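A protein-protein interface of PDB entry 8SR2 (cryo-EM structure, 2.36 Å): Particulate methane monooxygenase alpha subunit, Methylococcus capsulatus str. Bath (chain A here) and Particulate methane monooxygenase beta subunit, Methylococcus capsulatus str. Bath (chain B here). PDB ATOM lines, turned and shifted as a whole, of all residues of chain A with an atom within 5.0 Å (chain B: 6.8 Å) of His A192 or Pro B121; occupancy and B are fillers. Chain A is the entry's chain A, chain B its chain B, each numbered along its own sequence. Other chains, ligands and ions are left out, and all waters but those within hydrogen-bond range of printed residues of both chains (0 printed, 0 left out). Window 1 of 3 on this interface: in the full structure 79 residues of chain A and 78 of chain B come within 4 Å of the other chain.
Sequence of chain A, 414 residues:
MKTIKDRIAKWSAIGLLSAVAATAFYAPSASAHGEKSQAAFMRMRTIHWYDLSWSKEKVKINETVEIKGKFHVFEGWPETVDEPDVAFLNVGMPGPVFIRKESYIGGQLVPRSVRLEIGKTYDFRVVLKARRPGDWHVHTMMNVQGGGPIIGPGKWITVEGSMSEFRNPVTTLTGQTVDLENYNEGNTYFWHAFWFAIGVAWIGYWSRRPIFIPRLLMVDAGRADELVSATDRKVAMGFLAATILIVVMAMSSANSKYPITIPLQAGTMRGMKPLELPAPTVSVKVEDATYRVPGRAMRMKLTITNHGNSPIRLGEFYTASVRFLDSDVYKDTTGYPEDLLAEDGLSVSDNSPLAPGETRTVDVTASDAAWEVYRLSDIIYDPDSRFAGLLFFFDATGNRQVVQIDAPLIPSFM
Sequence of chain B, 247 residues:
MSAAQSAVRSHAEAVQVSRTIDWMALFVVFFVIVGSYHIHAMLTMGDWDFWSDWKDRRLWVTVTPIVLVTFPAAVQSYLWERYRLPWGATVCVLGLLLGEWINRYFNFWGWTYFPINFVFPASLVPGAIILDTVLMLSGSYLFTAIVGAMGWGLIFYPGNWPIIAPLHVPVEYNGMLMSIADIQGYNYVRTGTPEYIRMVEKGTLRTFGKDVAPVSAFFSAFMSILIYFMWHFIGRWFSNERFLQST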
ATOM      1  N   THR A 188       6.570  22.179 -19.490  1.00  0.00           N
ATOM      2  CA  THR A 188       6.291  22.216 -20.919  1.00  0.00           C
ATOM      3  C   THR A 188       4.989  22.958 -21.181  1.00  0.00           C
ATOM      4  O   THR A 188       4.900  23.768 -22.101  1.00  0.00           O
ATOM      5  CB  THR A 188       6.175  20.799 -21.507  1.00  0.00           C
ATOM      6  OG1 THR A 188       7.410  20.100 -21.316  1.00  0.00           O
ATOM      7  CG2 THR A 188       5.860  20.865 -22.991  1.00  0.00           C
ATOM      8  N   TYR A 189       3.983  22.675 -20.362  1.00  0.00           N
ATOM      9  CA  TYR A 189       2.681  23.312 -20.497  1.00  0.00           C
ATOM     10  C   TYR A 189       2.772  24.808 -20.226  1.00  0.00           C
ATOM     11  O   TYR A 189       2.268  25.619 -20.997  1.00  0.00           O
ATOM     12  CB  TYR A 189       1.680  22.680 -19.533  1.00  0.00           C
ATOM     13  CG  TYR A 189       0.997  21.450 -20.080  1.00  0.00           C
ATOM     14  CD1 TYR A 189       0.621  21.376 -21.410  1.00  0.00           C
ATOM     15  CD2 TYR A 189       0.729  20.362 -19.261  1.00  0.00           C
ATOM     16  CE1 TYR A 189      -0.005  20.251 -21.915  1.00  0.00           C
ATOM     17  CE2 TYR A 189       0.104  19.235 -19.756  1.00  0.00           C
ATOM     18  CZ  TYR A 189      -0.261  19.186 -21.083  1.00  0.00           C
ATOM     19  OH  TYR A 189      -0.884  18.065 -21.579  1.00  0.00           O
ATOM     20  N   PHE A 190       3.420  25.161 -19.123  1.00  0.00           N
ATOM     21  CA  PHE A 190       3.569  26.559 -18.739  1.00  0.00           C
ATOM     22  C   PHE A 190       4.152  27.416 -19.855  1.00  0.00           C
ATOM     23  O   PHE A 190       3.553  28.409 -20.261  1.00  0.00           O
ATOM     24  CB  PHE A 190       4.438  26.681 -17.486  1.00  0.00           C
ATOM     25  CG  PHE A 190       4.891  28.082 -17.204  1.00  0.00           C
ATOM     26  CD1 PHE A 190       4.052  28.979 -16.566  1.00  0.00           C
ATOM     27  CD2 PHE A 190       6.154  28.507 -17.577  1.00  0.00           C
ATOM     28  CE1 PHE A 190       4.463  30.272 -16.306  1.00  0.00           C
ATOM     29  CE2 PHE A 190       6.572  29.797 -17.321  1.00  0.00           C
ATOM     30  CZ  PHE A 190       5.727  30.681 -16.684  1.00  0.00           C
ATOM     31  N   TRP A 191       5.320  27.027 -20.348  1.00  0.00           N
ATOM     32  CA  TRP A 191       5.985  27.785 -21.402  1.00  0.00           C
ATOM     33  C   TRP A 191       5.150  27.924 -22.665  1.00  0.00           C
ATOM     34  O   TRP A 191       5.108  28.996 -23.265  1.00  0.00           O
ATOM     35  CB  TRP A 191       7.356  27.192 -21.715  1.00  0.00           C
ATOM     36  CG  TRP A 191       8.398  27.627 -20.744  1.00  0.00           C
ATOM     37  CD1 TRP A 191       9.171  26.828 -19.960  1.00  0.00           C
ATOM     38  CD2 TRP A 191       8.776  28.974 -20.439  1.00  0.00           C
ATOM     39  NE1 TRP A 191      10.010  27.591 -19.187  1.00  0.00           N
ATOM     40  CE2 TRP A 191       9.788  28.913 -19.465  1.00  0.00           C
ATOM     41  CE3 TRP A 191       8.358  30.225 -20.902  1.00  0.00           C
ATOM     42  CZ2 TRP A 191      10.390  30.054 -18.943  1.00  0.00           C
ATOM     43  CZ3 TRP A 191       8.956  31.356 -20.382  1.00  0.00           C
ATOM     44  CH2 TRP A 191       9.960  31.264 -19.413  1.00  0.00           C
ATOM     45  N   HIS A 192       4.487  26.850 -23.078  1.00  0.00           N
ATOM     46  CA  HIS A 192       3.663  26.921 -24.279  1.00  0.00           C
ATOM     47  C   HIS A 192       2.450  27.817 -24.060  1.00  0.00           C
ATOM     48  O   HIS A 192       2.104  28.624 -24.932  1.00  0.00           O
ATOM     49  CB  HIS A 192       3.236  25.517 -24.707  1.00  0.00           C
ATOM     50  CG  HIS A 192       4.164  24.884 -25.695  1.00  0.00           C
ATOM     51  ND1 HIS A 192       4.140  25.189 -27.040  1.00  0.00           N
ATOM     52  CD2 HIS A 192       5.146  23.966 -25.536  1.00  0.00           C
ATOM     53  CE1 HIS A 192       5.067  24.486 -27.665  1.00  0.00           C
ATOM     54  NE2 HIS A 192       5.690  23.734 -26.774  1.00  0.00           N
ATOM     55  N   ALA A 193       1.821  27.689 -22.901  1.00  0.00           N
ATOM     56  CA  ALA A 193       0.660  28.505 -22.577  1.00  0.00           C
ATOM     57  C   ALA A 193       1.078  29.962 -22.448  1.00  0.00           C
ATOM     58  O   ALA A 193       0.340  30.868 -22.831  1.00  0.00           O
ATOM     59  CB  ALA A 193       0.012  28.022 -21.290  1.00  0.00           C
ATOM     60  N   PHE A 194       2.273  30.179 -21.912  1.00  0.00           N
ATOM     61  CA  PHE A 194       2.799  31.525 -21.728  1.00  0.00           C
ATOM     62  C   PHE A 194       2.996  32.232 -23.064  1.00  0.00           C
ATOM     63  O   PHE A 194       2.619  33.389 -23.224  1.00  0.00           O
ATOM     64  CB  PHE A 194       4.118  31.483 -20.958  1.00  0.00           C
ATOM     65  CG  PHE A 194       4.827  32.802 -20.901  1.00  0.00           C
ATOM     66  CD1 PHE A 194       4.518  33.727 -19.918  1.00  0.00           C
ATOM     67  CD2 PHE A 194       5.805  33.119 -21.829  1.00  0.00           C
ATOM     68  CE1 PHE A 194       5.170  34.943 -19.861  1.00  0.00           C
ATOM     69  CE2 PHE A 194       6.461  34.334 -21.777  1.00  0.00           C
ATOM     70  CZ  PHE A 194       6.143  35.246 -20.792  1.00  0.00           C
ATOM     71  N   TRP A 195       3.592  31.530 -24.023  1.00  0.00           N
ATOM     72  CA  TRP A 195       3.833  32.108 -25.339  1.00  0.00           C
ATOM     73  C   TRP A 195       2.534  32.280 -26.119  1.00  0.00           C
ATOM     74  O   TRP A 195       2.318  33.316 -26.743  1.00  0.00           O
ATOM     75  CB  TRP A 195       4.860  31.285 -26.116  1.00  0.00           C
ATOM     76  CG  TRP A 195       6.250  31.508 -25.616  1.00  0.00           C
ATOM     77  CD1 TRP A 195       7.106  30.570 -25.123  1.00  0.00           C
ATOM     78  CD2 TRP A 195       6.940  32.761 -25.540  1.00  0.00           C
ATOM     79  NE1 TRP A 195       8.290  31.158 -24.752  1.00  0.00           N
ATOM     80  CE2 TRP A 195       8.214  32.503 -24.999  1.00  0.00           C
ATOM     81  CE3 TRP A 195       6.606  34.074 -25.883  1.00  0.00           C
ATOM     82  CZ2 TRP A 195       9.153  33.509 -24.792  1.00  0.00           C
ATOM     83  CZ3 TRP A 195       7.540  35.069 -25.678  1.00  0.00           C
ATOM     84  CH2 TRP A 195       8.798  34.783 -25.139  1.00  0.00           C
ATOM     85  N   PHE A 196       1.669  31.275 -26.067  1.00  0.00           N
ATOM     86  CA  PHE A 196       0.397  31.361 -26.760  1.00  0.00           C
ATOM     87  C   PHE A 196      -0.368  32.566 -26.230  1.00  0.00           C
ATOM     88  O   PHE A 196      -1.048  33.259 -26.980  1.00  0.00           O
ATOM     89  CB  PHE A 196      -0.420  30.087 -26.572  1.00  0.00           C
ATOM     90  CG  PHE A 196      -1.417  29.845 -27.663  1.00  0.00           C
ATOM     91  CD1 PHE A 196      -2.688  30.387 -27.588  1.00  0.00           C
ATOM     92  CD2 PHE A 196      -1.084  29.084 -28.768  1.00  0.00           C
ATOM     93  CE1 PHE A 196      -3.609  30.171 -28.594  1.00  0.00           C
ATOM     94  CE2 PHE A 196      -1.998  28.862 -29.778  1.00  0.00           C
ATOM     95  CZ  PHE A 196      -3.264  29.406 -29.690  1.00  0.00           C
ATOM     96  N   ALA A 197      -0.235  32.818 -24.933  1.00  0.00           N
ATOM     97  CA  ALA A 197      -0.902  33.948 -24.303  1.00  0.00           C
ATOM     98  C   ALA A 197      -0.362  35.255 -24.866  1.00  0.00           C
ATOM     99  O   ALA A 197      -1.121  36.176 -25.158  1.00  0.00           O
ATOM    100  CB  ALA A 197      -0.717  33.903 -22.795  1.00  0.00           C
ATOM    101  N   ASP B  49       9.273  17.840 -34.736  1.00  0.00           N
ATOM    102  CA  ASP B  49       8.295  18.446 -33.837  1.00  0.00           C
ATOM    103  C   ASP B  49       7.463  17.410 -33.087  1.00  0.00           C
ATOM    104  O   ASP B  49       6.686  17.748 -32.197  1.00  0.00           O
ATOM    105  CB  ASP B  49       7.373  19.379 -34.622  1.00  0.00           C
ATOM    106  CG  ASP B  49       6.632  20.347 -33.730  1.00  0.00           C
ATOM    107  OD1 ASP B  49       7.295  21.155 -33.045  1.00  0.00           O
ATOM    108  OD2 ASP B  49       5.386  20.306 -33.713  1.00  0.00           O
ATOM    109  N   PHE B  50       7.639  16.147 -33.451  1.00  0.00           N
ATOM    110  CA  PHE B  50       6.908  15.042 -32.839  1.00  0.00           C
ATOM    111  C   PHE B  50       7.596  14.540 -31.578  1.00  0.00           C
ATOM    112  O   PHE B  50       6.927  14.221 -30.589  1.00  0.00           O
ATOM    113  CB  PHE B  50       6.747  13.897 -33.841  1.00  0.00           C
ATOM    114  CG  PHE B  50       5.590  14.067 -34.782  1.00  0.00           C
ATOM    115  CD1 PHE B  50       4.668  15.082 -34.594  1.00  0.00           C
ATOM    116  CD2 PHE B  50       5.420  13.204 -35.851  1.00  0.00           C
ATOM    117  CE1 PHE B  50       3.603  15.239 -35.460  1.00  0.00           C
ATOM    118  CE2 PHE B  50       4.356  13.355 -36.721  1.00  0.00           C
ATOM    119  CZ  PHE B  50       3.447  14.374 -36.524  1.00  0.00           C
ATOM    120  N   LYS B  55      14.359  16.462 -30.966  1.00  0.00           N
ATOM    121  CA  LYS B  55      14.691  17.884 -30.848  1.00  0.00           C
ATOM    122  C   LYS B  55      16.181  18.017 -30.542  1.00  0.00           C
ATOM    123  O   LYS B  55      16.605  18.207 -29.398  1.00  0.00           O
ATOM    124  CB  LYS B  55      13.847  18.553 -29.771  1.00  0.00           C
ATOM    125  CG  LYS B  55      12.380  18.177 -29.787  1.00  0.00           C
ATOM    126  CD  LYS B  55      11.544  19.211 -30.519  1.00  0.00           C
ATOM    127  CE  LYS B  55      10.111  19.215 -30.016  1.00  0.00           C
ATOM    128  NZ  LYS B  55       9.434  17.916 -30.269  1.00  0.00           N
ATOM    129  N   TRP B  60      17.166  19.868 -36.137  1.00  0.00           N
ATOM    130  CA  TRP B  60      15.920  20.522 -35.749  1.00  0.00           C
ATOM    131  C   TRP B  60      16.053  22.038 -35.828  1.00  0.00           C
ATOM    132  O   TRP B  60      15.261  22.715 -36.499  1.00  0.00           O
ATOM    133  CB  TRP B  60      15.540  20.068 -34.336  1.00  0.00           C
ATOM    134  CG  TRP B  60      14.357  20.742 -33.722  1.00  0.00           C
ATOM    135  CD1 TRP B  60      13.113  20.876 -34.261  1.00  0.00           C
ATOM    136  CD2 TRP B  60      14.302  21.354 -32.429  1.00  0.00           C
ATOM    137  NE1 TRP B  60      12.288  21.545 -33.388  1.00  0.00           N
ATOM    138  CE2 TRP B  60      12.997  21.849 -32.256  1.00  0.00           C
ATOM    139  CE3 TRP B  60      15.236  21.536 -31.404  1.00  0.00           C
ATOM    140  CZ2 TRP B  60      12.600  22.515 -31.098  1.00  0.00           C
ATOM    141  CZ3 TRP B  60      14.841  22.196 -30.257  1.00  0.00           C
ATOM    142  CH2 TRP B  60      13.535  22.679 -30.113  1.00  0.00           C
ATOM    143  N   LEU B  96      -0.778  27.229 -36.155  1.00  0.00           N
ATOM    144  CA  LEU B  96       0.005  26.001 -36.206  1.00  0.00           C
ATOM    145  C   LEU B  96       0.145  25.386 -34.822  1.00  0.00           C
ATOM    146  O   LEU B  96      -0.012  24.170 -34.656  1.00  0.00           O
ATOM    147  CB  LEU B  96       1.382  26.279 -36.810  1.00  0.00           C
ATOM    148  CG  LEU B  96       2.327  25.079 -36.918  1.00  0.00           C
ATOM    149  CD1 LEU B  96       1.658  23.925 -37.645  1.00  0.00           C
ATOM    150  CD2 LEU B  96       3.624  25.472 -37.605  1.00  0.00           C
ATOM    151  N   LEU B  97       0.419  26.214 -33.812  1.00  0.00           N
ATOM    152  CA  LEU B  97       0.558  25.711 -32.451  1.00  0.00           C
ATOM    153  C   LEU B  97      -0.752  25.136 -31.932  1.00  0.00           C
ATOM    154  O   LEU B  97      -0.755  24.098 -31.264  1.00  0.00           O
ATOM    155  CB  LEU B  97       1.057  26.825 -31.530  1.00  0.00           C
ATOM    156  CG  LEU B  97       2.562  27.086 -31.565  1.00  0.00           C
ATOM    157  CD1 LEU B  97       2.891  28.418 -30.913  1.00  0.00           C
ATOM    158  CD2 LEU B  97       3.303  25.954 -30.880  1.00  0.00           C
ATOM    159  N   GLU B 100      -1.348  21.776 -33.704  1.00  0.00           N
ATOM    160  CA  GLU B 100      -0.387  20.797 -33.216  1.00  0.00           C
ATOM    161  C   GLU B 100      -0.736  20.340 -31.807  1.00  0.00           C
ATOM    162  O   GLU B 100      -0.736  19.142 -31.521  1.00  0.00           O
ATOM    163  CB  GLU B 100       1.024  21.387 -33.257  1.00  0.00           C
ATOM    164  CG  GLU B 100       1.885  20.856 -34.388  1.00  0.00           C
ATOM    165  CD  GLU B 100       3.012  21.802 -34.754  1.00  0.00           C
ATOM    166  OE1 GLU B 100       3.143  22.856 -34.098  1.00  0.00           O
ATOM    167  OE2 GLU B 100       3.767  21.491 -35.700  1.00  0.00           O
ATOM    168  N   TRP B 101      -1.041  21.285 -30.926  1.00  0.00           N
ATOM    169  CA  TRP B 101      -1.386  20.935 -29.554  1.00  0.00           C
ATOM    170  C   TRP B 101      -2.665  20.113 -29.485  1.00  0.00           C
ATOM    171  O   TRP B 101      -2.797  19.230 -28.641  1.00  0.00           O
ATOM    172  CB  TRP B 101      -1.493  22.185 -28.684  1.00  0.00           C
ATOM    173  CG  TRP B 101      -0.233  22.477 -27.944  1.00  0.00           C
ATOM    174  CD1 TRP B 101       0.571  23.566 -28.095  1.00  0.00           C
ATOM    175  CD2 TRP B 101       0.383  21.659 -26.944  1.00  0.00           C
ATOM    176  NE1 TRP B 101       1.647  23.481 -27.248  1.00  0.00           N
ATOM    177  CE2 TRP B 101       1.555  22.319 -26.529  1.00  0.00           C
ATOM    178  CE3 TRP B 101       0.056  20.434 -26.357  1.00  0.00           C
ATOM    179  CZ2 TRP B 101       2.400  21.797 -25.555  1.00  0.00           C
ATOM    180  CZ3 TRP B 101       0.897  19.918 -25.389  1.00  0.00           C
ATOM    181  CH2 TRP B 101       2.053  20.597 -24.998  1.00  0.00           C
ATOM    182  N   ARG B 104      -1.661  16.757 -30.456  1.00  0.00           N
ATOM    183  CA  ARG B 104      -0.748  16.226 -29.453  1.00  0.00           C
ATOM    184  C   ARG B 104      -1.507  15.676 -28.256  1.00  0.00           C
ATOM    185  O   ARG B 104      -1.127  14.665 -27.675  1.00  0.00           O
ATOM    186  CB  ARG B 104       0.188  17.328 -28.958  1.00  0.00           C
ATOM    187  CG  ARG B 104       1.446  17.544 -29.777  1.00  0.00           C
ATOM    188  CD  ARG B 104       1.697  16.429 -30.773  1.00  0.00           C
ATOM    189  NE  ARG B 104       2.951  16.658 -31.481  1.00  0.00           N
ATOM    190  CZ  ARG B 104       3.046  17.342 -32.615  1.00  0.00           C
ATOM    191  NH1 ARG B 104       1.958  17.846 -33.173  1.00  0.00           N
ATOM    192  NH2 ARG B 104       4.225  17.512 -33.193  1.00  0.00           N
ATOM    193  N   ILE B 116       2.743  13.477 -23.002  1.00  0.00           N
ATOM    194  CA  ILE B 116       2.789  14.843 -23.517  1.00  0.00           C
ATOM    195  C   ILE B 116       4.205  15.399 -23.443  1.00  0.00           C
ATOM    196  O   ILE B 116       4.665  16.087 -24.362  1.00  0.00           O
ATOM    197  CB  ILE B 116       1.788  15.729 -22.757  1.00  0.00           C
ATOM    198  CG1 ILE B 116       0.366  15.184 -22.915  1.00  0.00           C
ATOM    199  CG2 ILE B 116       1.883  17.174 -23.226  1.00  0.00           C
ATOM    200  CD1 ILE B 116      -0.376  15.731 -24.120  1.00  0.00           C
ATOM    201  N   VAL B 119       5.804  14.069 -26.557  1.00  0.00           N
ATOM    202  CA  VAL B 119       5.305  14.462 -27.870  1.00  0.00           C
ATOM    203  C   VAL B 119       4.937  15.946 -27.921  1.00  0.00           C
ATOM    204  O   VAL B 119       4.141  16.354 -28.762  1.00  0.00           O
ATOM    205  CB  VAL B 119       4.123  13.582 -28.307  1.00  0.00           C
ATOM    206  CG1 VAL B 119       4.551  12.128 -28.389  1.00  0.00           C
ATOM    207  CG2 VAL B 119       2.946  13.750 -27.355  1.00  0.00           C
ATOM    208  N   PHE B 120       5.512  16.768 -27.047  1.00  0.00           N
ATOM    209  CA  PHE B 120       5.201  18.188 -27.061  1.00  0.00           C
ATOM    210  C   PHE B 120       5.752  18.854 -28.323  1.00  0.00           C
ATOM    211  O   PHE B 120       6.783  18.438 -28.858  1.00  0.00           O
ATOM    212  CB  PHE B 120       5.776  18.874 -25.826  1.00  0.00           C
ATOM    213  CG  PHE B 120       7.277  18.864 -25.771  1.00  0.00           C
ATOM    214  CD1 PHE B 120       7.956  17.787 -25.229  1.00  0.00           C
ATOM    215  CD2 PHE B 120       8.011  19.936 -26.252  1.00  0.00           C
ATOM    216  CE1 PHE B 120       9.333  17.776 -25.176  1.00  0.00           C
ATOM    217  CE2 PHE B 120       9.389  19.929 -26.204  1.00  0.00           C
ATOM    218  CZ  PHE B 120      10.051  18.847 -25.664  1.00  0.00           C
ATOM    219  N   PRO B 121       5.079  19.887 -28.822  1.00  0.00           N
ATOM    220  CA  PRO B 121       5.586  20.621 -29.985  1.00  0.00           C
ATOM    221  C   PRO B 121       6.585  21.699 -29.580  1.00  0.00           C
ATOM    222  O   PRO B 121       6.862  21.926 -28.402  1.00  0.00           O
ATOM    223  CB  PRO B 121       4.318  21.238 -30.582  1.00  0.00           C
ATOM    224  CG  PRO B 121       3.439  21.454 -29.404  1.00  0.00           C
ATOM    225  CD  PRO B 121       3.726  20.326 -28.440  1.00  0.00           C
ATOM    226  N   ALA B 122       7.149  22.358 -30.586  1.00  0.00           N
ATOM    227  CA  ALA B 122       8.130  23.410 -30.358  1.00  0.00           C
ATOM    228  C   ALA B 122       7.469  24.780 -30.277  1.00  0.00           C
ATOM    229  O   ALA B 122       6.437  25.017 -30.901  1.00  0.00           O
ATOM    230  CB  ALA B 122       9.183  23.395 -31.452  1.00  0.00           C
ATOM    231  N   SER B 123       8.071  25.676 -29.506  1.00  0.00           N
ATOM    232  CA  SER B 123       7.551  27.027 -29.349  1.00  0.00           C
ATOM    233  C   SER B 123       8.081  27.915 -30.464  1.00  0.00           C
ATOM    234  O   SER B 123       9.280  27.928 -30.737  1.00  0.00           O
ATOM    235  CB  SER B 123       7.950  27.595 -27.987  1.00  0.00           C
ATOM    236  OG  SER B 123       7.419  28.893 -27.803  1.00  0.00           O
ATOM    237  N   LEU B 124       7.188  28.654 -31.114  1.00  0.00           N
ATOM    238  CA  LEU B 124       7.586  29.534 -32.206  1.00  0.00           C
ATOM    239  C   LEU B 124       7.020  30.943 -32.066  1.00  0.00           C
ATOM    240  O   LEU B 124       7.135  31.753 -32.982  1.00  0.00           O
ATOM    241  CB  LEU B 124       7.154  28.947 -33.552  1.00  0.00           C
ATOM    242  CG  LEU B 124       7.093  27.425 -33.678  1.00  0.00           C
ATOM    243  CD1 LEU B 124       5.778  26.995 -34.310  1.00  0.00           C
ATOM    244  CD2 LEU B 124       8.272  26.913 -34.489  1.00  0.00           C
ATOM    245  N   VAL B 125       6.417  31.236 -30.922  1.00  0.00           N
ATOM    246  CA  VAL B 125       5.829  32.553 -30.699  1.00  0.00           C
ATOM    247  C   VAL B 125       6.843  33.691 -30.800  1.00  0.00           C
ATOM    248  O   VAL B 125       6.619  34.647 -31.538  1.00  0.00           O
ATOM    249  CB  VAL B 125       5.086  32.633 -29.356  1.00  0.00           C
ATOM    250  CG1 VAL B 125       4.785  34.082 -29.011  1.00  0.00           C
ATOM    251  CG2 VAL B 125       3.801  31.825 -29.420  1.00  0.00           C
ATOM    252  N   ASN B 160      13.077  27.735 -27.223  1.00  0.00           N
ATOM    253  CA  ASN B 160      12.695  26.393 -26.810  1.00  0.00           C
ATOM    254  C   ASN B 160      13.606  25.813 -25.736  1.00  0.00           C
ATOM    255  O   ASN B 160      13.301  24.741 -25.203  1.00  0.00           O
ATOM    256  CB  ASN B 160      12.682  25.450 -28.019  1.00  0.00           C
ATOM    257  CG  ASN B 160      11.513  25.709 -28.944  1.00  0.00           C
ATOM    258  OD1 ASN B 160      10.456  25.095 -28.811  1.00  0.00           O
ATOM    259  ND2 ASN B 160      11.699  26.616 -29.894  1.00  0.00           N
ATOM    260  N   ILE B 163      12.194  24.680 -22.277  1.00  0.00           N
ATOM    261  CA  ILE B 163      11.396  23.461 -22.330  1.00  0.00           C
ATOM    262  C   ILE B 163      12.209  22.177 -22.462  1.00  0.00           C
ATOM    263  O   ILE B 163      12.013  21.234 -21.698  1.00  0.00           O
ATOM    264  CB  ILE B 163      10.372  23.518 -23.479  1.00  0.00           C
ATOM    265  CG1 ILE B 163       9.457  24.731 -23.312  1.00  0.00           C
ATOM    266  CG2 ILE B 163       9.559  22.237 -23.532  1.00  0.00           C
ATOM    267  CD1 ILE B 163       8.925  25.276 -24.619  1.00  0.00           C
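Of the 10 printed residues of chain A, 5 touch a printed residue of chain B. Hydrophobic or aromatic side chains of chain B that line the printed part of chain A: Leu B97, Trp B101, Ile B116, Phe B120, Pro B121, Val B125 and Ile B163. Among the printed residues, no Asp or Glu carboxylate lies within 4 Å of a Lys or Arg side-chain nitrogen of the other chain.
Thr A188 touches Phe B120. Ile B163 touches Thr A188 (CG2 to OG1, 3.8 Å). Tyr A189 touches Trp B101. Ile B116 touches Tyr A189. Trp A191 touches Ile B163. His A192 touches Leu B97. CE1 of His A192 touches O of Ala B122 (3.6 Å). His A192 touches Ser B123. Ser B123 touches Trp A195 (OG to CD1, 3.2 Å). Val B125 touches Trp A195.
A ring nitrogen (ND1) of His A192 sits at hydrogen-bond distance from the indole nitrogen (NE1) of Trp B101 (3.0 Å). O of Pro B121 lies within hydrogen-bond range of NE2 of His A192.
Of the printed residues of chain B, Thr A188 touches Phe B120 and Ile B163. Of chain B, only Leu B97, Trp B101, Pro B121, Ala B122 and Ser B123 come within 4 Å of His A192. Leu B96 touches none of the printed residues of chain A. Of the printed residues of chain A, Phe B120 touches Thr A188. Of chain A, only His A192 (2.7 Å) comes within 4 Å of Pro B121. Printed residues of chain A within 4 Å of Ser B123: His A192 and Trp A195. Of the printed residues of chain A, Val B125 touches Trp A195 (3.4 Å). The nearest residue of chain B that does not touch His A192 is Ile B163 (4.1 Å). The nearest printed residue of chain A that does not touch Val B125 is Phe A196 (4.01 Å).
N of Ser B123 lies within hydrogen-bond range of OD1 of Asn B160. The backbone carbonyl oxygen (O) of Phe B120 sits at hydrogen-bond distance from the side-chain amino group (NZ) of Lys B55. The side-chain carboxylate of Asp B49 lies within hydrogen-bond range of the backbone NH of Ala B122, 2.7 Å away.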
